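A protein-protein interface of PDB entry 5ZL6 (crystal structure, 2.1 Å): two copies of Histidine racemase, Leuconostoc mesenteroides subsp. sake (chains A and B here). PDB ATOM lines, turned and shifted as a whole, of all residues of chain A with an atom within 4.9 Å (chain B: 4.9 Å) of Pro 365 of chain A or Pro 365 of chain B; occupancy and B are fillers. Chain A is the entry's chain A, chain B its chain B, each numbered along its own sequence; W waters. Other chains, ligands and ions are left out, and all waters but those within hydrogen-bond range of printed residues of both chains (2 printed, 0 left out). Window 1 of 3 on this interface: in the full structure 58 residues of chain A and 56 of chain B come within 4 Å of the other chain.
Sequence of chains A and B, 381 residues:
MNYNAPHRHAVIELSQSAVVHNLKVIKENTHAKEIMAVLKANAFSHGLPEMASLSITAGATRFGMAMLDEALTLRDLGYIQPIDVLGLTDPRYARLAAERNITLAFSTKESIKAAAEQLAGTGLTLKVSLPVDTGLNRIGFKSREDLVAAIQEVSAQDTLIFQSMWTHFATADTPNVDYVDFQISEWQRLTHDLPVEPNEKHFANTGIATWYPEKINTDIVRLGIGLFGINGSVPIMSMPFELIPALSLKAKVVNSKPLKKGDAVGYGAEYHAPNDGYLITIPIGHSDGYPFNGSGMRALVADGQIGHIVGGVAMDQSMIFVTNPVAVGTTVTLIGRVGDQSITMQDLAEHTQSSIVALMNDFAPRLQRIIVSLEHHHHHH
Among the printed residues, merely in contact across the chains: Pro 365 of chain A with Tyr 3 of chain B (3.3 Å), Tyr 3 of chain A with Pro 365 of chain B (3.3 Å), Tyr 3 of chain A with Tyr 3 of chain B (3.3 Å), Asn 42 of chain A with Tyr 3 of chain B (3.8 Å), Tyr 3 of chain A with Asn 42 of chain B (3.8 Å) and Pro 365 of chain A with Pro 365 of chain B (3.96 Å).
Tyr 3 of chain B touches its own counterpart, Tyr 3 of chain A.
Tyr 3 of chain A touches Asn 42 of chain B, and with the chains exchanged Asn 42 of chain A touches Tyr 3 of chain B.
Tyr 3 of chain A touches Pro 365 of chain B, and with the chains exchanged Pro 365 of chain A touches Tyr 3 of chain B.
Pro 365 of chain A touches its own counterpart, Pro 365 of chain B.
Of the 6 pairs that touch across the chains among the printed residues, 6 have their exchanged pair printed and touching as well.
Pro 365 of chain A touches just these residues of chain B: Tyr 3 and Pro 365.
Of chain A, only Tyr 3 (3.3 Å) and Pro 365 (3.96 Å) come within 4 Å of Pro 365 of chain B.
Of the printed residues of chain A, Asn 42 of chain B touches Tyr 3 (3.8 Å).
Printed residues of chain A within 4 Å of Tyr 3 of chain B: Tyr 3 (3.3 Å), Asn 42 (3.8 Å) and Pro 365 (3.3 Å).
Leu 367 of chain A touches none of the printed residues of chain B.
Arg 366 of chain A touches none of the printed residues of chain B.
Water W2 bridges OH of Tyr 3 of chain B (2.6 Å) and ND2 of Asn 42 of chain A (3.1 Å).
Water W1 lies within hydrogen-bond range of ND2 of Asn 42 of chain B and OH of Tyr 3 of chain A.
N of Asn 4 of chain A sits close to O of Pro 365 of chain A, 3.4 Å away.
O of Pro 365 of chain B lies close to N of Asn 4 of chain B.
Printed residues of chain B that touch a printed residue of chain A: Tyr 3, Asn 42 and Pro 365.
Hydrophobic or aromatic side chains of chain B within 4 Å of the printed part of chain A: Tyr 3 and Pro 365.
Hydrophobic or aromatic side chains of chain A that line the printed part of chain B: Tyr 3 and Pro 365.
Among the printed residues, 6 pairs touch across the chains.
Among the printed residues, no Asp or Glu carboxylate lies within 4 Å of a Lys or Arg side-chain nitrogen of the other chain.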
ATOM      1  N   TYR A   3      12.227 -16.945  13.312  1.00  0.00           N
ATOM      2  CA  TYR A   3      13.507 -17.037  12.620  1.00  0.00           C
ATOM      3  C   TYR A   3      14.619 -17.381  13.601  1.00  0.00           C
ATOM      4  O   TYR A   3      15.494 -18.189  13.298  1.00  0.00           O
ATOM      5  CB  TYR A   3      13.840 -15.734  11.886  1.00  0.00           C
ATOM      6  CG  TYR A   3      13.192 -15.607  10.524  1.00  0.00           C
ATOM      7  CD1 TYR A   3      13.727 -16.249   9.413  1.00  0.00           C
ATOM      8  CD2 TYR A   3      12.051 -14.841  10.347  1.00  0.00           C
ATOM      9  CE1 TYR A   3      13.136 -16.133   8.163  1.00  0.00           C
ATOM     10  CE2 TYR A   3      11.455 -14.717   9.104  1.00  0.00           C
ATOM     11  CZ  TYR A   3      11.999 -15.365   8.017  1.00  0.00           C
ATOM     12  OH  TYR A   3      11.404 -15.238   6.781  1.00  0.00           O
ATOM     13  N   ASN A   4      14.581 -16.770  14.781  1.00  0.00           N
ATOM     14  CA  ASN A   4      15.633 -16.981  15.762  1.00  0.00           C
ATOM     15  C   ASN A   4      15.603 -18.408  16.301  1.00  0.00           C
ATOM     16  O   ASN A   4      14.561 -19.068  16.295  1.00  0.00           O
ATOM     17  CB  ASN A   4      15.516 -15.969  16.907  1.00  0.00           C
ATOM     18  CG  ASN A   4      14.235 -16.127  17.704  1.00  0.00           C
ATOM     19  OD1 ASN A   4      13.232 -16.624  17.196  1.00  0.00           O
ATOM     20  ND2 ASN A   4      14.263 -15.700  18.961  1.00  0.00           N
ATOM     21  N   ALA A   5      16.757 -18.893  16.744  1.00  0.00           N
ATOM     22  CA  ALA A   5      16.837 -20.241  17.282  1.00  0.00           C
ATOM     23  C   ALA A   5      17.298 -20.211  18.730  1.00  0.00           C
ATOM     24  O   ALA A   5      18.488 -20.359  19.002  1.00  0.00           O
ATOM     25  CB  ALA A   5      17.765 -21.090  16.447  1.00  0.00           C
ATOM     26  N   ASN A  42      16.675  -4.245   9.854  1.00  0.00           N
ATOM     27  CA  ASN A  42      16.703  -4.927  11.142  1.00  0.00           C
ATOM     28  C   ASN A  42      17.770  -4.343  12.058  1.00  0.00           C
ATOM     29  O   ASN A  42      18.471  -5.078  12.751  1.00  0.00           O
ATOM     30  CB  ASN A  42      16.935  -6.431  10.951  1.00  0.00           C
ATOM     31  CG  ASN A  42      16.787  -7.223  12.251  1.00  0.00           C
ATOM     32  OD1 ASN A  42      16.046  -6.831  13.155  1.00  0.00           O
ATOM     33  ND2 ASN A  42      17.493  -8.344  12.342  1.00  0.00           N
ATOM     34  N   PHE A 363      24.536 -10.186   9.581  1.00  0.00           N
ATOM     35  CA  PHE A 363      24.003 -11.094  10.599  1.00  0.00           C
ATOM     36  C   PHE A 363      22.525 -11.403  10.374  1.00  0.00           C
ATOM     37  O   PHE A 363      21.693 -10.501  10.328  1.00  0.00           O
ATOM     38  CB  PHE A 363      24.215 -10.520  12.000  1.00  0.00           C
ATOM     39  CG  PHE A 363      25.654 -10.256  12.329  1.00  0.00           C
ATOM     40  CD1 PHE A 363      26.533 -11.306  12.548  1.00  0.00           C
ATOM     41  CD2 PHE A 363      26.136  -8.960  12.403  1.00  0.00           C
ATOM     42  CE1 PHE A 363      27.862 -11.069  12.840  1.00  0.00           C
ATOM     43  CE2 PHE A 363      27.464  -8.711  12.696  1.00  0.00           C
ATOM     44  CZ  PHE A 363      28.329  -9.768  12.914  1.00  0.00           C
ATOM     45  N   ALA A 364      22.218 -12.688  10.232  1.00  0.00           N
ATOM     46  CA  ALA A 364      20.853 -13.168  10.023  1.00  0.00           C
ATOM     47  C   ALA A 364      20.053 -13.199  11.331  1.00  0.00           C
ATOM     48  O   ALA A 364      20.629 -13.211  12.418  1.00  0.00           O
ATOM     49  CB  ALA A 364      20.883 -14.556   9.388  1.00  0.00           C
ATOM     50  N   PRO A 365      18.715 -13.197  11.227  1.00  0.00           N
ATOM     51  CA  PRO A 365      17.873 -13.324  12.423  1.00  0.00           C
ATOM     52  C   PRO A 365      17.910 -14.711  13.082  1.00  0.00           C
ATOM     53  O   PRO A 365      17.301 -14.878  14.136  1.00  0.00           O
ATOM     54  CB  PRO A 365      16.464 -13.023  11.894  1.00  0.00           C
ATOM     55  CG  PRO A 365      16.540 -13.220  10.426  1.00  0.00           C
ATOM     56  CD  PRO A 365      17.929 -12.823  10.041  1.00  0.00           C
ATOM     57  N   ARG A 366      18.602 -15.685  12.498  1.00  0.00           N
ATOM     58  CA  ARG A 366      18.585 -17.033  13.071  1.00  0.00           C
ATOM     59  C   ARG A 366      19.321 -17.076  14.405  1.00  0.00           C
ATOM     60  O   ARG A 366      19.024 -17.914  15.255  1.00  0.00           O
ATOM     61  CB  ARG A 366      19.187 -18.058  12.113  1.00  0.00           C
ATOM     62  CG  ARG A 366      19.041 -19.489  12.610  1.00  0.00           C
ATOM     63  CD  ARG A 366      19.420 -20.514  11.551  1.00  0.00           C
ATOM     64  NE  ARG A 366      20.839 -20.469  11.203  1.00  0.00           N
ATOM     65  CZ  ARG A 366      21.426 -21.315  10.362  1.00  0.00           C
ATOM     66  NH1 ARG A 366      20.718 -22.278   9.786  1.00  0.00           N
ATOM     67  NH2 ARG A 366      22.721 -21.204  10.097  1.00  0.00           N
ATOM     68  N   LEU A 367      20.270 -16.162  14.581  1.00  0.00           N
ATOM     69  CA  LEU A 367      20.988 -16.009  15.842  1.00  0.00           C
ATOM     70  C   LEU A 367      20.110 -15.391  16.933  1.00  0.00           C
ATOM     71  O   LEU A 367      19.449 -14.376  16.715  1.00  0.00           O
ATOM     72  CB  LEU A 367      22.239 -15.148  15.637  1.00  0.00           C
ATOM     73  CG  LEU A 367      23.419 -15.804  14.918  1.00  0.00           C
ATOM     74  CD1 LEU A 367      24.300 -14.759  14.250  1.00  0.00           C
ATOM     75  CD2 LEU A 367      24.234 -16.642  15.897  1.00  0.00           C
ATOM     76  N   ARG A 369      19.333 -13.158  20.029  1.00  0.00           N
ATOM     77  CA  ARG A 369      19.887 -11.920  20.586  1.00  0.00           C
ATOM     78  C   ARG A 369      19.738 -11.827  22.104  1.00  0.00           C
ATOM     79  O   ARG A 369      18.744 -12.276  22.669  1.00  0.00           O
ATOM     80  CB  ARG A 369      19.221 -10.697  19.951  1.00  0.00           C
ATOM     81  CG  ARG A 369      19.890 -10.175  18.689  1.00  0.00           C
ATOM     82  CD  ARG A 369      19.712 -11.110  17.503  1.00  0.00           C
ATOM     83  NE  ARG A 369      20.221 -10.494  16.280  1.00  0.00           N
ATOM     84  CZ  ARG A 369      20.281 -11.101  15.098  1.00  0.00           C
ATOM     85  NH1 ARG A 369      19.866 -12.354  14.966  1.00  0.00           N
ATOM     86  NH2 ARG A 369      20.763 -10.451  14.046  1.00  0.00           N
ATOM     87  N   TYR B   3       9.257  -9.601   9.307  1.00  0.00           N
ATOM     88  CA  TYR B   3      10.525  -9.332   8.636  1.00  0.00           C
ATOM     89  C   TYR B   3      10.315  -8.906   7.182  1.00  0.00           C
ATOM     90  O   TYR B   3      10.948  -7.963   6.706  1.00  0.00           O
ATOM     91  CB  TYR B   3      11.446 -10.554   8.699  1.00  0.00           C
ATOM     92  CG  TYR B   3      12.299 -10.603   9.950  1.00  0.00           C
ATOM     93  CD1 TYR B   3      13.341  -9.703  10.140  1.00  0.00           C
ATOM     94  CD2 TYR B   3      12.064 -11.548  10.937  1.00  0.00           C
ATOM     95  CE1 TYR B   3      14.121  -9.742  11.282  1.00  0.00           C
ATOM     96  CE2 TYR B   3      12.840 -11.600  12.079  1.00  0.00           C
ATOM     97  CZ  TYR B   3      13.866 -10.695  12.247  1.00  0.00           C
ATOM     98  OH  TYR B   3      14.634 -10.745  13.387  1.00  0.00           O
ATOM     99  N   ASN B   4       9.424  -9.597   6.479  1.00  0.00           N
ATOM    100  CA  ASN B   4       9.209  -9.329   5.063  1.00  0.00           C
ATOM    101  C   ASN B   4       8.558  -7.970   4.820  1.00  0.00           C
ATOM    102  O   ASN B   4       7.794  -7.482   5.657  1.00  0.00           O
ATOM    103  CB  ASN B   4       8.354 -10.430   4.442  1.00  0.00           C
ATOM    104  CG  ASN B   4       6.990 -10.531   5.083  1.00  0.00           C
ATOM    105  OD1 ASN B   4       6.863 -10.494   6.308  1.00  0.00           O
ATOM    106  ND2 ASN B   4       5.957 -10.642   4.260  1.00  0.00           N
ATOM    107  N   ALA B   5       8.846  -7.374   3.666  1.00  0.00           N
ATOM    108  CA  ALA B   5       8.338  -6.042   3.339  1.00  0.00           C
ATOM    109  C   ALA B   5       7.314  -6.073   2.202  1.00  0.00           C
ATOM    110  O   ALA B   5       7.627  -5.712   1.065  1.00  0.00           O
ATOM    111  CB  ALA B   5       9.495  -5.120   2.981  1.00  0.00           C
ATOM    112  N   ASN B  42      16.794 -20.993   6.558  1.00  0.00           N
ATOM    113  CA  ASN B  42      15.665 -20.443   5.822  1.00  0.00           C
ATOM    114  C   ASN B  42      15.714 -20.917   4.378  1.00  0.00           C
ATOM    115  O   ASN B  42      15.562 -20.126   3.451  1.00  0.00           O
ATOM    116  CB  ASN B  42      15.670 -18.914   5.886  1.00  0.00           C
ATOM    117  CG  ASN B  42      14.442 -18.299   5.247  1.00  0.00           C
ATOM    118  OD1 ASN B  42      13.379 -18.925   5.179  1.00  0.00           O
ATOM    119  ND2 ASN B  42      14.580 -17.064   4.775  1.00  0.00           N
ATOM    120  N   PHE B 363      20.409 -13.885   0.977  1.00  0.00           N
ATOM    121  CA  PHE B 363      19.165 -13.117   0.888  1.00  0.00           C
ATOM    122  C   PHE B 363      18.437 -12.970   2.224  1.00  0.00           C
ATOM    123  O   PHE B 363      18.160 -13.955   2.912  1.00  0.00           O
ATOM    124  CB  PHE B 363      18.243 -13.748  -0.153  1.00  0.00           C
ATOM    125  CG  PHE B 363      18.807 -13.709  -1.542  1.00  0.00           C
ATOM    126  CD1 PHE B 363      18.824 -12.525  -2.260  1.00  0.00           C
ATOM    127  CD2 PHE B 363      19.339 -14.847  -2.120  1.00  0.00           C
ATOM    128  CE1 PHE B 363      19.353 -12.481  -3.537  1.00  0.00           C
ATOM    129  CE2 PHE B 363      19.870 -14.811  -3.393  1.00  0.00           C
ATOM    130  CZ  PHE B 363      19.879 -13.627  -4.104  1.00  0.00           C
ATOM    131  N   ALA B 364      18.129 -11.725   2.579  1.00  0.00           N
ATOM    132  CA  ALA B 364      17.437 -11.420   3.826  1.00  0.00           C
ATOM    133  C   ALA B 364      15.937 -11.682   3.712  1.00  0.00           C
ATOM    134  O   ALA B 364      15.374 -11.625   2.620  1.00  0.00           O
ATOM    135  CB  ALA B 364      17.690  -9.979   4.224  1.00  0.00           C
ATOM    136  N   PRO B 365      15.284 -11.974   4.844  1.00  0.00           N
ATOM    137  CA  PRO B 365      13.828 -12.166   4.818  1.00  0.00           C
ATOM    138  C   PRO B 365      13.051 -10.868   4.578  1.00  0.00           C
ATOM    139  O   PRO B 365      11.824 -10.914   4.442  1.00  0.00           O
ATOM    140  CB  PRO B 365      13.524 -12.737   6.207  1.00  0.00           C
ATOM    141  CG  PRO B 365      14.671 -12.330   7.055  1.00  0.00           C
ATOM    142  CD  PRO B 365      15.862 -12.315   6.154  1.00  0.00           C
ATOM    143  N   ARG B 366      13.743  -9.733   4.517  1.00  0.00           N
ATOM    144  CA  ARG B 366      13.067  -8.468   4.258  1.00  0.00           C
ATOM    145  C   ARG B 366      12.424  -8.457   2.876  1.00  0.00           C
ATOM    146  O   ARG B 366      11.423  -7.779   2.665  1.00  0.00           O
ATOM    147  CB  ARG B 366      14.024  -7.288   4.393  1.00  0.00           C
ATOM    148  CG  ARG B 366      13.306  -5.951   4.368  1.00  0.00           C
ATOM    149  CD  ARG B 366      14.230  -4.788   4.668  1.00  0.00           C
ATOM    150  NE  ARG B 366      15.239  -4.591   3.634  1.00  0.00           N
ATOM    151  CZ  ARG B 366      16.149  -3.625   3.670  1.00  0.00           C
ATOM    152  NH1 ARG B 366      16.164  -2.773   4.686  1.00  0.00           N
ATOM    153  NH2 ARG B 366      17.047  -3.510   2.700  1.00  0.00           N
ATOM    154  N   LEU B 367      12.998  -9.203   1.938  1.00  0.00           N
ATOM    155  CA  LEU B 367      12.420  -9.328   0.602  1.00  0.00           C
ATOM    156  C   LEU B 367      11.161 -10.182   0.602  1.00  0.00           C
ATOM    157  O   LEU B 367      11.129 -11.256   1.201  1.00  0.00           O
ATOM    158  CB  LEU B 367      13.430  -9.929  -0.373  1.00  0.00           C
ATOM    159  CG  LEU B 367      14.567  -9.036  -0.865  1.00  0.00           C
ATOM    160  CD1 LEU B 367      15.694  -9.893  -1.424  1.00  0.00           C
ATOM    161  CD2 LEU B 367      14.057  -8.072  -1.917  1.00  0.00           C
ATOM    162  N   ARG B 369       8.666 -12.834  -0.721  1.00  0.00           N
ATOM    163  CA  ARG B 369       8.698 -14.016  -1.579  1.00  0.00           C
ATOM    164  C   ARG B 369       7.380 -14.213  -2.320  1.00  0.00           C
ATOM    165  O   ARG B 369       6.305 -13.933  -1.794  1.00  0.00           O
ATOM    166  CB  ARG B 369       9.016 -15.277  -0.773  1.00  0.00           C
ATOM    167  CG  ARG B 369      10.492 -15.598  -0.651  1.00  0.00           C
ATOM    168  CD  ARG B 369      11.207 -14.580   0.218  1.00  0.00           C
ATOM    169  NE  ARG B 369      12.595 -14.950   0.487  1.00  0.00           N
ATOM    170  CZ  ARG B 369      13.444 -14.190   1.170  1.00  0.00           C
ATOM    171  NH1 ARG B 369      13.051 -13.016   1.645  1.00  0.00           N
ATOM    172  NH2 ARG B 369      14.686 -14.601   1.381  1.00  0.00           N
HETATM  173  O   HOH W   1      12.136 -15.688   3.966  1.00  0.00           O
HETATM  174  O   HOH W   2      16.893 -10.267  14.658  1.00  0.00           O
